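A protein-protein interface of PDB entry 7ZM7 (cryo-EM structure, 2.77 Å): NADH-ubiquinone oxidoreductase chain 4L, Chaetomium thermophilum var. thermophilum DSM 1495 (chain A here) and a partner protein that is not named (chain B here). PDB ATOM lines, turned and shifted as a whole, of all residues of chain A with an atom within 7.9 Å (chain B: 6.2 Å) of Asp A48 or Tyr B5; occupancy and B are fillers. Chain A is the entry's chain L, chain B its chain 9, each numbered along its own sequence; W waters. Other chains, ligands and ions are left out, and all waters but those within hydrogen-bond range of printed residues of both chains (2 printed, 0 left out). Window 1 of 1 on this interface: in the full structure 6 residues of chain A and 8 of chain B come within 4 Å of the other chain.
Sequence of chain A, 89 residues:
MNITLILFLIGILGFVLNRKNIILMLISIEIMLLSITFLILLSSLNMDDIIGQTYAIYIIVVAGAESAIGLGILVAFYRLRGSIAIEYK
The backbone NH (N) of Ile A50 lies within hydrogen-bond range of the backbone carbonyl oxygen (O) of Tyr B5, at 3.2 Å.
O of Asn A46 is in hydrogen-bond range of NH1 of Arg B13.
The backbone carbonyl oxygen of Pro B11 sits close to the side-chain carboxylate of Asp A48 (3.5 Å).
The side-chain carboxylate of Asp A48 lies within hydrogen-bond range of the backbone NH of Leu B7, 3.1 Å away.
OG of Ser B3 sits at hydrogen-bond distance from OD1 of Asp A49, 2.5 Å away.
OD1 of Asp A49 lies close to O of Tyr B5, at 2.9 Å.
N of Gly B4 lies within hydrogen-bond range of OG of Ser B12, 2.9 Å away.
O of Ser A44 lies within hydrogen-bond range of N of Asp A49, at 3.2 Å.
OG of Ser B3 is in hydrogen-bond range of N of Tyr B5, 3.0 Å away.
The backbone carbonyl oxygen (O) of Leu A42 lies close to the side-chain amide oxygen (OD1) of Asn A46 (3.2 Å).
Arg B13 touches Met A47.
Tyr B5 touches Asp A48 (O to O, 3.7 Å).
Asp A48 touches Gly B6 (O to CA, 3.1 Å).
Asp A48 touches Ser B12 (O to CB, 3.6 Å).
Asp A48 touches Arg B13.
Leu B7 touches Asp A49 (CD2 to O, 3.4 Å).
Ile A50 touches Gly B6 (CB to O, 3.8 Å).
CD1 of Ile A50 touches CD2 of Leu B7, 3.9 Å away.
Gln A53 touches Leu B7.
Asp A48 touches six residues of chain B.
Of chain A, only Asp A48, Asp A49 and Ile A50 come within 4 Å of Tyr B5.
Gly B4 touches none of the printed residues of chain A.
Gly B6 touches just these residues of chain A: Asp A48 and Ile A50.
Printed residues of chain B within 4 Å of Asp A49: Ser B3 (2.5 Å), Tyr B5 (2.9 Å) and Leu B7 (3.4 Å).
Printed residues of chain A within 4 Å of Leu B7: Asp A48, Asp A49, Ile A50 and Gln A53.
Printed residues of chain B within 4 Å of Met A47: Arg B13 (3.4 Å).
Of the printed residues of chain A, Ser B12 touches Asp A48 (3.6 Å).
Gly A52 touches none of the printed residues of chain B.
The nearest residue of chain A that does not touch Tyr B5 is Ile A51 (4.9 Å).
The nearest printed residue of chain A that does not touch Ser B12 is Asp A49 (4.4 Å).
Hydrophobic or aromatic side chains of chain B within 4 Å of the printed part of chain A: Tyr B5 and Leu B7.
Of the 12 printed residues of chain A, 6 touch a printed residue of chain B.
Hydrophobic or aromatic side chains of chain A that line the printed part of chain B: Ile A50.
Water W1 lies within hydrogen-bond range of O of Asn A46 (2.7 Å), O of Leu A45 (3.2 Å) and NE of Arg B13 (3.4 Å).
Water W2 bridges the side-chain carboxylate of Asp A48 (2.8 Å) and the side-chain amide oxygen of Asn B8 (3.4 Å).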
ATOM      1  N   LEU A  42      -9.131  -3.037  14.997  1.00  0.00           N
ATOM      2  CA  LEU A  42     -10.533  -3.417  14.856  1.00  0.00           C
ATOM      3  C   LEU A  42     -11.183  -3.663  16.204  1.00  0.00           C
ATOM      4  O   LEU A  42     -12.353  -3.337  16.401  1.00  0.00           O
ATOM      5  CB  LEU A  42     -10.660  -4.642  13.961  1.00  0.00           C
ATOM      6  CG  LEU A  42     -11.069  -4.340  12.530  1.00  0.00           C
ATOM      7  CD1 LEU A  42     -10.052  -3.467  11.862  1.00  0.00           C
ATOM      8  CD2 LEU A  42     -11.198  -5.642  11.811  1.00  0.00           C
ATOM      9  N   SER A  43     -10.403  -4.067  17.193  1.00  0.00           N
ATOM     10  CA  SER A  43     -10.968  -4.235  18.554  1.00  0.00           C
ATOM     11  C   SER A  43     -11.103  -2.875  19.236  1.00  0.00           C
ATOM     12  O   SER A  43     -12.021  -2.711  20.043  1.00  0.00           O
ATOM     13  CB  SER A  43     -10.123  -5.182  19.338  1.00  0.00           C
ATOM     14  OG  SER A  43      -9.836  -6.335  18.566  1.00  0.00           O
ATOM     15  N   SER A  44     -10.233  -1.931  18.906  1.00  0.00           N
ATOM     16  CA  SER A  44     -10.345  -0.554  19.453  1.00  0.00           C
ATOM     17  C   SER A  44     -11.639   0.118  18.985  1.00  0.00           C
ATOM     18  O   SER A  44     -12.264   0.796  19.799  1.00  0.00           O
ATOM     19  CB  SER A  44      -9.149   0.227  19.036  1.00  0.00           C
ATOM     20  OG  SER A  44      -7.977  -0.530  19.249  1.00  0.00           O
ATOM     21  N   LEU A  45     -12.022  -0.065  17.722  1.00  0.00           N
ATOM     22  CA  LEU A  45     -13.296   0.480  17.189  1.00  0.00           C
ATOM     23  C   LEU A  45     -14.447  -0.148  17.971  1.00  0.00           C
ATOM     24  O   LEU A  45     -15.388   0.566  18.304  1.00  0.00           O
ATOM     25  CB  LEU A  45     -13.375   0.117  15.702  1.00  0.00           C
ATOM     26  CG  LEU A  45     -14.546   0.722  14.938  1.00  0.00           C
ATOM     27  CD1 LEU A  45     -14.429   2.237  14.895  1.00  0.00           C
ATOM     28  CD2 LEU A  45     -14.626   0.148  13.534  1.00  0.00           C
ATOM     29  N   ASN A  46     -14.353  -1.431  18.276  1.00  0.00           N
ATOM     30  CA  ASN A  46     -15.395  -2.157  19.050  1.00  0.00           C
ATOM     31  C   ASN A  46     -15.545  -1.628  20.471  1.00  0.00           C
ATOM     32  O   ASN A  46     -16.677  -1.670  20.957  1.00  0.00           O
ATOM     33  CB  ASN A  46     -15.136  -3.659  19.098  1.00  0.00           C
ATOM     34  CG  ASN A  46     -15.157  -4.313  17.736  1.00  0.00           C
ATOM     35  OD1 ASN A  46     -15.483  -3.679  16.736  1.00  0.00           O
ATOM     36  ND2 ASN A  46     -14.810  -5.587  17.688  1.00  0.00           N
ATOM     37  N   MET A  47     -14.480  -1.135  21.111  1.00  0.00           N
ATOM     38  CA  MET A  47     -14.562  -0.791  22.556  1.00  0.00           C
ATOM     39  C   MET A  47     -14.559   0.727  22.752  1.00  0.00           C
ATOM     40  O   MET A  47     -14.606   1.154  23.912  1.00  0.00           O
ATOM     41  CB  MET A  47     -13.418  -1.434  23.341  1.00  0.00           C
ATOM     42  CG  MET A  47     -13.213  -2.915  23.086  1.00  0.00           C
ATOM     43  SD  MET A  47     -11.738  -3.551  23.944  1.00  0.00           S
ATOM     44  CE  MET A  47     -10.538  -2.282  23.547  1.00  0.00           C
ATOM     45  N   ASP A  48     -14.541   1.509  21.670  1.00  0.00           N
ATOM     46  CA  ASP A  48     -14.516   2.997  21.738  1.00  0.00           C
ATOM     47  C   ASP A  48     -13.276   3.475  22.490  1.00  0.00           C
ATOM     48  O   ASP A  48     -13.399   4.411  23.296  1.00  0.00           O
ATOM     49  CB  ASP A  48     -15.788   3.572  22.361  1.00  0.00           C
ATOM     50  CG  ASP A  48     -15.819   5.090  22.355  1.00  0.00           C
ATOM     51  OD1 ASP A  48     -15.466   5.675  21.312  1.00  0.00           O
ATOM     52  OD2 ASP A  48     -16.183   5.677  23.396  1.00  0.00           O
ATOM     53  N   ASP A  49     -12.134   2.841  22.246  1.00  0.00           N
ATOM     54  CA  ASP A  49     -10.886   3.202  22.968  1.00  0.00           C
ATOM     55  C   ASP A  49      -9.870   3.814  22.000  1.00  0.00           C
ATOM     56  O   ASP A  49      -9.656   3.244  20.926  1.00  0.00           O
ATOM     57  CB  ASP A  49     -10.351   2.020  23.779  1.00  0.00           C
ATOM     58  CG  ASP A  49      -9.544   2.439  24.995  1.00  0.00           C
ATOM     59  OD1 ASP A  49      -9.395   3.659  25.206  1.00  0.00           O
ATOM     60  OD2 ASP A  49      -9.073   1.542  25.728  1.00  0.00           O
ATOM     61  N   ILE A  50      -9.248   4.919  22.394  1.00  0.00           N
ATOM     62  CA  ILE A  50      -8.223   5.585  21.548  1.00  0.00           C
ATOM     63  C   ILE A  50      -6.842   4.977  21.809  1.00  0.00           C
ATOM     64  O   ILE A  50      -5.938   5.233  21.011  1.00  0.00           O
ATOM     65  CB  ILE A  50      -8.252   7.101  21.829  1.00  0.00           C
ATOM     66  CG1 ILE A  50      -7.769   7.928  20.635  1.00  0.00           C
ATOM     67  CG2 ILE A  50      -7.510   7.444  23.108  1.00  0.00           C
ATOM     68  CD1 ILE A  50      -8.646   7.810  19.411  1.00  0.00           C
ATOM     69  N   ILE A  51      -6.688   4.218  22.899  1.00  0.00           N
ATOM     70  CA  ILE A  51      -5.350   3.674  23.273  1.00  0.00           C
ATOM     71  C   ILE A  51      -5.006   2.557  22.294  1.00  0.00           C
ATOM     72  O   ILE A  51      -3.809   2.369  22.023  1.00  0.00           O
ATOM     73  CB  ILE A  51      -5.292   3.235  24.751  1.00  0.00           C
ATOM     74  CG1 ILE A  51      -4.004   3.705  25.426  1.00  0.00           C
ATOM     75  CG2 ILE A  51      -5.498   1.738  24.912  1.00  0.00           C
ATOM     76  CD1 ILE A  51      -3.670   5.146  25.142  1.00  0.00           C
ATOM     77  N   GLY A  52      -6.018   1.855  21.779  1.00  0.00           N
ATOM     78  CA  GLY A  52      -5.730   0.869  20.760  1.00  0.00           C
ATOM     79  C   GLY A  52      -5.218   1.500  19.486  1.00  0.00           C
ATOM     80  O   GLY A  52      -4.363   0.939  18.805  1.00  0.00           O
ATOM     81  N   GLN A  53      -5.744   2.672  19.144  1.00  0.00           N
ATOM     82  CA  GLN A  53      -5.261   3.411  17.988  1.00  0.00           C
ATOM     83  C   GLN A  53      -3.822   3.849  18.171  1.00  0.00           C
ATOM     84  O   GLN A  53      -3.024   3.799  17.236  1.00  0.00           O
ATOM     85  CB  GLN A  53      -6.145   4.625  17.756  1.00  0.00           C
ATOM     86  CG  GLN A  53      -7.530   4.290  17.347  1.00  0.00           C
ATOM     87  CD  GLN A  53      -8.026   5.209  16.287  1.00  0.00           C
ATOM     88  OE1 GLN A  53      -7.275   5.614  15.419  1.00  0.00           O
ATOM     89  NE2 GLN A  53      -9.290   5.552  16.350  1.00  0.00           N
ATOM     90  N   ALA B   2     -11.232   0.457  29.115  1.00  0.00           N
ATOM     91  CA  ALA B   2     -10.523   0.612  30.412  1.00  0.00           C
ATOM     92  C   ALA B   2      -9.714   1.915  30.486  1.00  0.00           C
ATOM     93  O   ALA B   2      -9.519   2.405  31.595  1.00  0.00           O
ATOM     94  CB  ALA B   2      -9.708  -0.605  30.762  1.00  0.00           C
ATOM     95  N   SER B   3      -9.214   2.425  29.358  1.00  0.00           N
ATOM     96  CA  SER B   3      -8.342   3.633  29.363  1.00  0.00           C
ATOM     97  C   SER B   3      -9.057   4.887  29.880  1.00  0.00           C
ATOM     98  O   SER B   3      -8.424   5.620  30.646  1.00  0.00           O
ATOM     99  CB  SER B   3      -7.714   3.873  28.035  1.00  0.00           C
ATOM    100  OG  SER B   3      -8.478   4.787  27.272  1.00  0.00           O
ATOM    101  N   GLY B   4     -10.311   5.122  29.507  1.00  0.00           N
ATOM    102  CA  GLY B   4     -10.987   6.362  29.922  1.00  0.00           C
ATOM    103  C   GLY B   4     -11.073   7.362  28.794  1.00  0.00           C
ATOM    104  O   GLY B   4     -11.668   8.409  29.010  1.00  0.00           O
ATOM    105  N   TYR B   5     -10.448   7.078  27.655  1.00  0.00           N
ATOM    106  CA  TYR B   5     -10.413   8.018  26.510  1.00  0.00           C
ATOM    107  C   TYR B   5     -11.067   7.349  25.304  1.00  0.00           C
ATOM    108  O   TYR B   5     -10.620   6.276  24.894  1.00  0.00           O
ATOM    109  CB  TYR B   5      -8.990   8.551  26.314  1.00  0.00           C
ATOM    110  CG  TYR B   5      -8.360   9.062  27.582  1.00  0.00           C
ATOM    111  CD1 TYR B   5      -8.485  10.388  27.962  1.00  0.00           C
ATOM    112  CD2 TYR B   5      -7.669   8.209  28.423  1.00  0.00           C
ATOM    113  CE1 TYR B   5      -7.921  10.858  29.137  1.00  0.00           C
ATOM    114  CE2 TYR B   5      -7.107   8.658  29.604  1.00  0.00           C
ATOM    115  CZ  TYR B   5      -7.232   9.988  29.963  1.00  0.00           C
ATOM    116  OH  TYR B   5      -6.677  10.430  31.126  1.00  0.00           O
ATOM    117  N   GLY B   6     -12.084   7.981  24.731  1.00  0.00           N
ATOM    118  CA  GLY B   6     -12.795   7.399  23.584  1.00  0.00           C
ATOM    119  C   GLY B   6     -12.422   8.027  22.266  1.00  0.00           C
ATOM    120  O   GLY B   6     -11.574   8.918  22.269  1.00  0.00           O
ATOM    121  N   LEU B   7     -13.021   7.550  21.179  1.00  0.00           N
ATOM    122  CA  LEU B   7     -12.706   8.029  19.811  1.00  0.00           C
ATOM    123  C   LEU B   7     -13.104   9.488  19.566  1.00  0.00           C
ATOM    124  O   LEU B   7     -12.414  10.131  18.773  1.00  0.00           O
ATOM    125  CB  LEU B   7     -13.377   7.079  18.815  1.00  0.00           C
ATOM    126  CG  LEU B   7     -13.124   5.590  19.049  1.00  0.00           C
ATOM    127  CD1 LEU B   7     -13.839   4.751  18.005  1.00  0.00           C
ATOM    128  CD2 LEU B   7     -11.638   5.281  19.051  1.00  0.00           C
ATOM    129  N   ASN B   8     -14.159   9.989  20.205  1.00  0.00           N
ATOM    130  CA  ASN B   8     -14.722  11.331  19.903  1.00  0.00           C
ATOM    131  C   ASN B   8     -14.160  12.413  20.822  1.00  0.00           C
ATOM    132  O   ASN B   8     -14.718  13.525  20.830  1.00  0.00           O
ATOM    133  CB  ASN B   8     -16.246  11.318  20.015  1.00  0.00           C
ATOM    134  CG  ASN B   8     -16.723  11.232  21.447  1.00  0.00           C
ATOM    135  OD1 ASN B   8     -16.307  10.352  22.198  1.00  0.00           O
ATOM    136  ND2 ASN B   8     -17.593  12.147  21.835  1.00  0.00           N
ATOM    137  N   GLY B   9     -13.089  12.104  21.555  1.00  0.00           N
ATOM    138  CA  GLY B   9     -12.502  13.069  22.504  1.00  0.00           C
ATOM    139  C   GLY B   9     -13.078  12.897  23.896  1.00  0.00           C
ATOM    140  O   GLY B   9     -12.468  13.406  24.842  1.00  0.00           O
ATOM    141  N   GLY B  10     -14.228  12.232  24.011  1.00  0.00           N
ATOM    142  CA  GLY B  10     -14.863  11.982  25.309  1.00  0.00           C
ATOM    143  C   GLY B  10     -14.371  10.697  25.940  1.00  0.00           C
ATOM    144  O   GLY B  10     -13.395  10.137  25.447  1.00  0.00           O
ATOM    145  N   PRO B  11     -14.975  10.248  27.054  1.00  0.00           N
ATOM    146  CA  PRO B  11     -14.546   9.038  27.753  1.00  0.00           C
ATOM    147  C   PRO B  11     -14.919   7.713  27.065  1.00  0.00           C
ATOM    148  O   PRO B  11     -15.717   7.743  26.158  1.00  0.00           O
ATOM    149  CB  PRO B  11     -15.233   9.184  29.116  1.00  0.00           C
ATOM    150  CG  PRO B  11     -15.738  10.606  29.170  1.00  0.00           C
ATOM    151  CD  PRO B  11     -16.074  10.922  27.735  1.00  0.00           C
ATOM    152  N   SER B  12     -14.294   6.601  27.470  1.00  0.00           N
ATOM    153  CA  SER B  12     -14.568   5.280  26.835  1.00  0.00           C
ATOM    154  C   SER B  12     -15.872   4.662  27.364  1.00  0.00           C
ATOM    155  O   SER B  12     -16.152   4.845  28.546  1.00  0.00           O
ATOM    156  CB  SER B  12     -13.382   4.344  26.893  1.00  0.00           C
ATOM    157  OG  SER B  12     -12.813   4.304  28.188  1.00  0.00           O
ATOM    158  N   ARG B  13     -16.616   3.926  26.533  1.00  0.00           N
ATOM    159  CA  ARG B  13     -17.958   3.383  26.894  1.00  0.00           C
ATOM    160  C   ARG B  13     -17.930   2.431  28.089  1.00  0.00           C
ATOM    161  O   ARG B  13     -18.892   2.461  28.861  1.00  0.00           O
ATOM    162  CB  ARG B  13     -18.632   2.747  25.674  1.00  0.00           C
ATOM    163  CG  ARG B  13     -17.840   1.633  25.012  1.00  0.00           C
ATOM    164  CD  ARG B  13     -18.605   1.093  23.822  1.00  0.00           C
ATOM    165  NE  ARG B  13     -17.993  -0.145  23.380  1.00  0.00           N
ATOM    166  CZ  ARG B  13     -18.327  -1.332  23.852  1.00  0.00           C
ATOM    167  NH1 ARG B  13     -17.714  -2.416  23.415  1.00  0.00           N
ATOM    168  NH2 ARG B  13     -19.274  -1.425  24.766  1.00  0.00           N
ATOM    169  N   PHE B  15     -15.618   2.279  30.466  1.00  0.00           N
ATOM    170  CA  PHE B  15     -14.797   2.777  31.599  1.00  0.00           C
ATOM    171  C   PHE B  15     -15.609   2.833  32.904  1.00  0.00           C
ATOM    172  O   PHE B  15     -15.009   2.550  33.946  1.00  0.00           O
ATOM    173  CB  PHE B  15     -14.103   4.072  31.182  1.00  0.00           C
ATOM    174  CG  PHE B  15     -13.191   4.694  32.206  1.00  0.00           C
ATOM    175  CD1 PHE B  15     -11.966   4.124  32.494  1.00  0.00           C
ATOM    176  CD2 PHE B  15     -13.539   5.869  32.848  1.00  0.00           C
ATOM    177  CE1 PHE B  15     -11.109   4.707  33.411  1.00  0.00           C
ATOM    178  CE2 PHE B  15     -12.683   6.449  33.767  1.00  0.00           C
ATOM    179  CZ  PHE B  15     -11.469   5.868  34.044  1.00  0.00           C
HETATM  180  O   HOH W   1     -18.076   0.374  19.977  1.00  0.00           O
HETATM  181  O   HOH W   2     -16.978   7.718  20.127  1.00  0.00           O
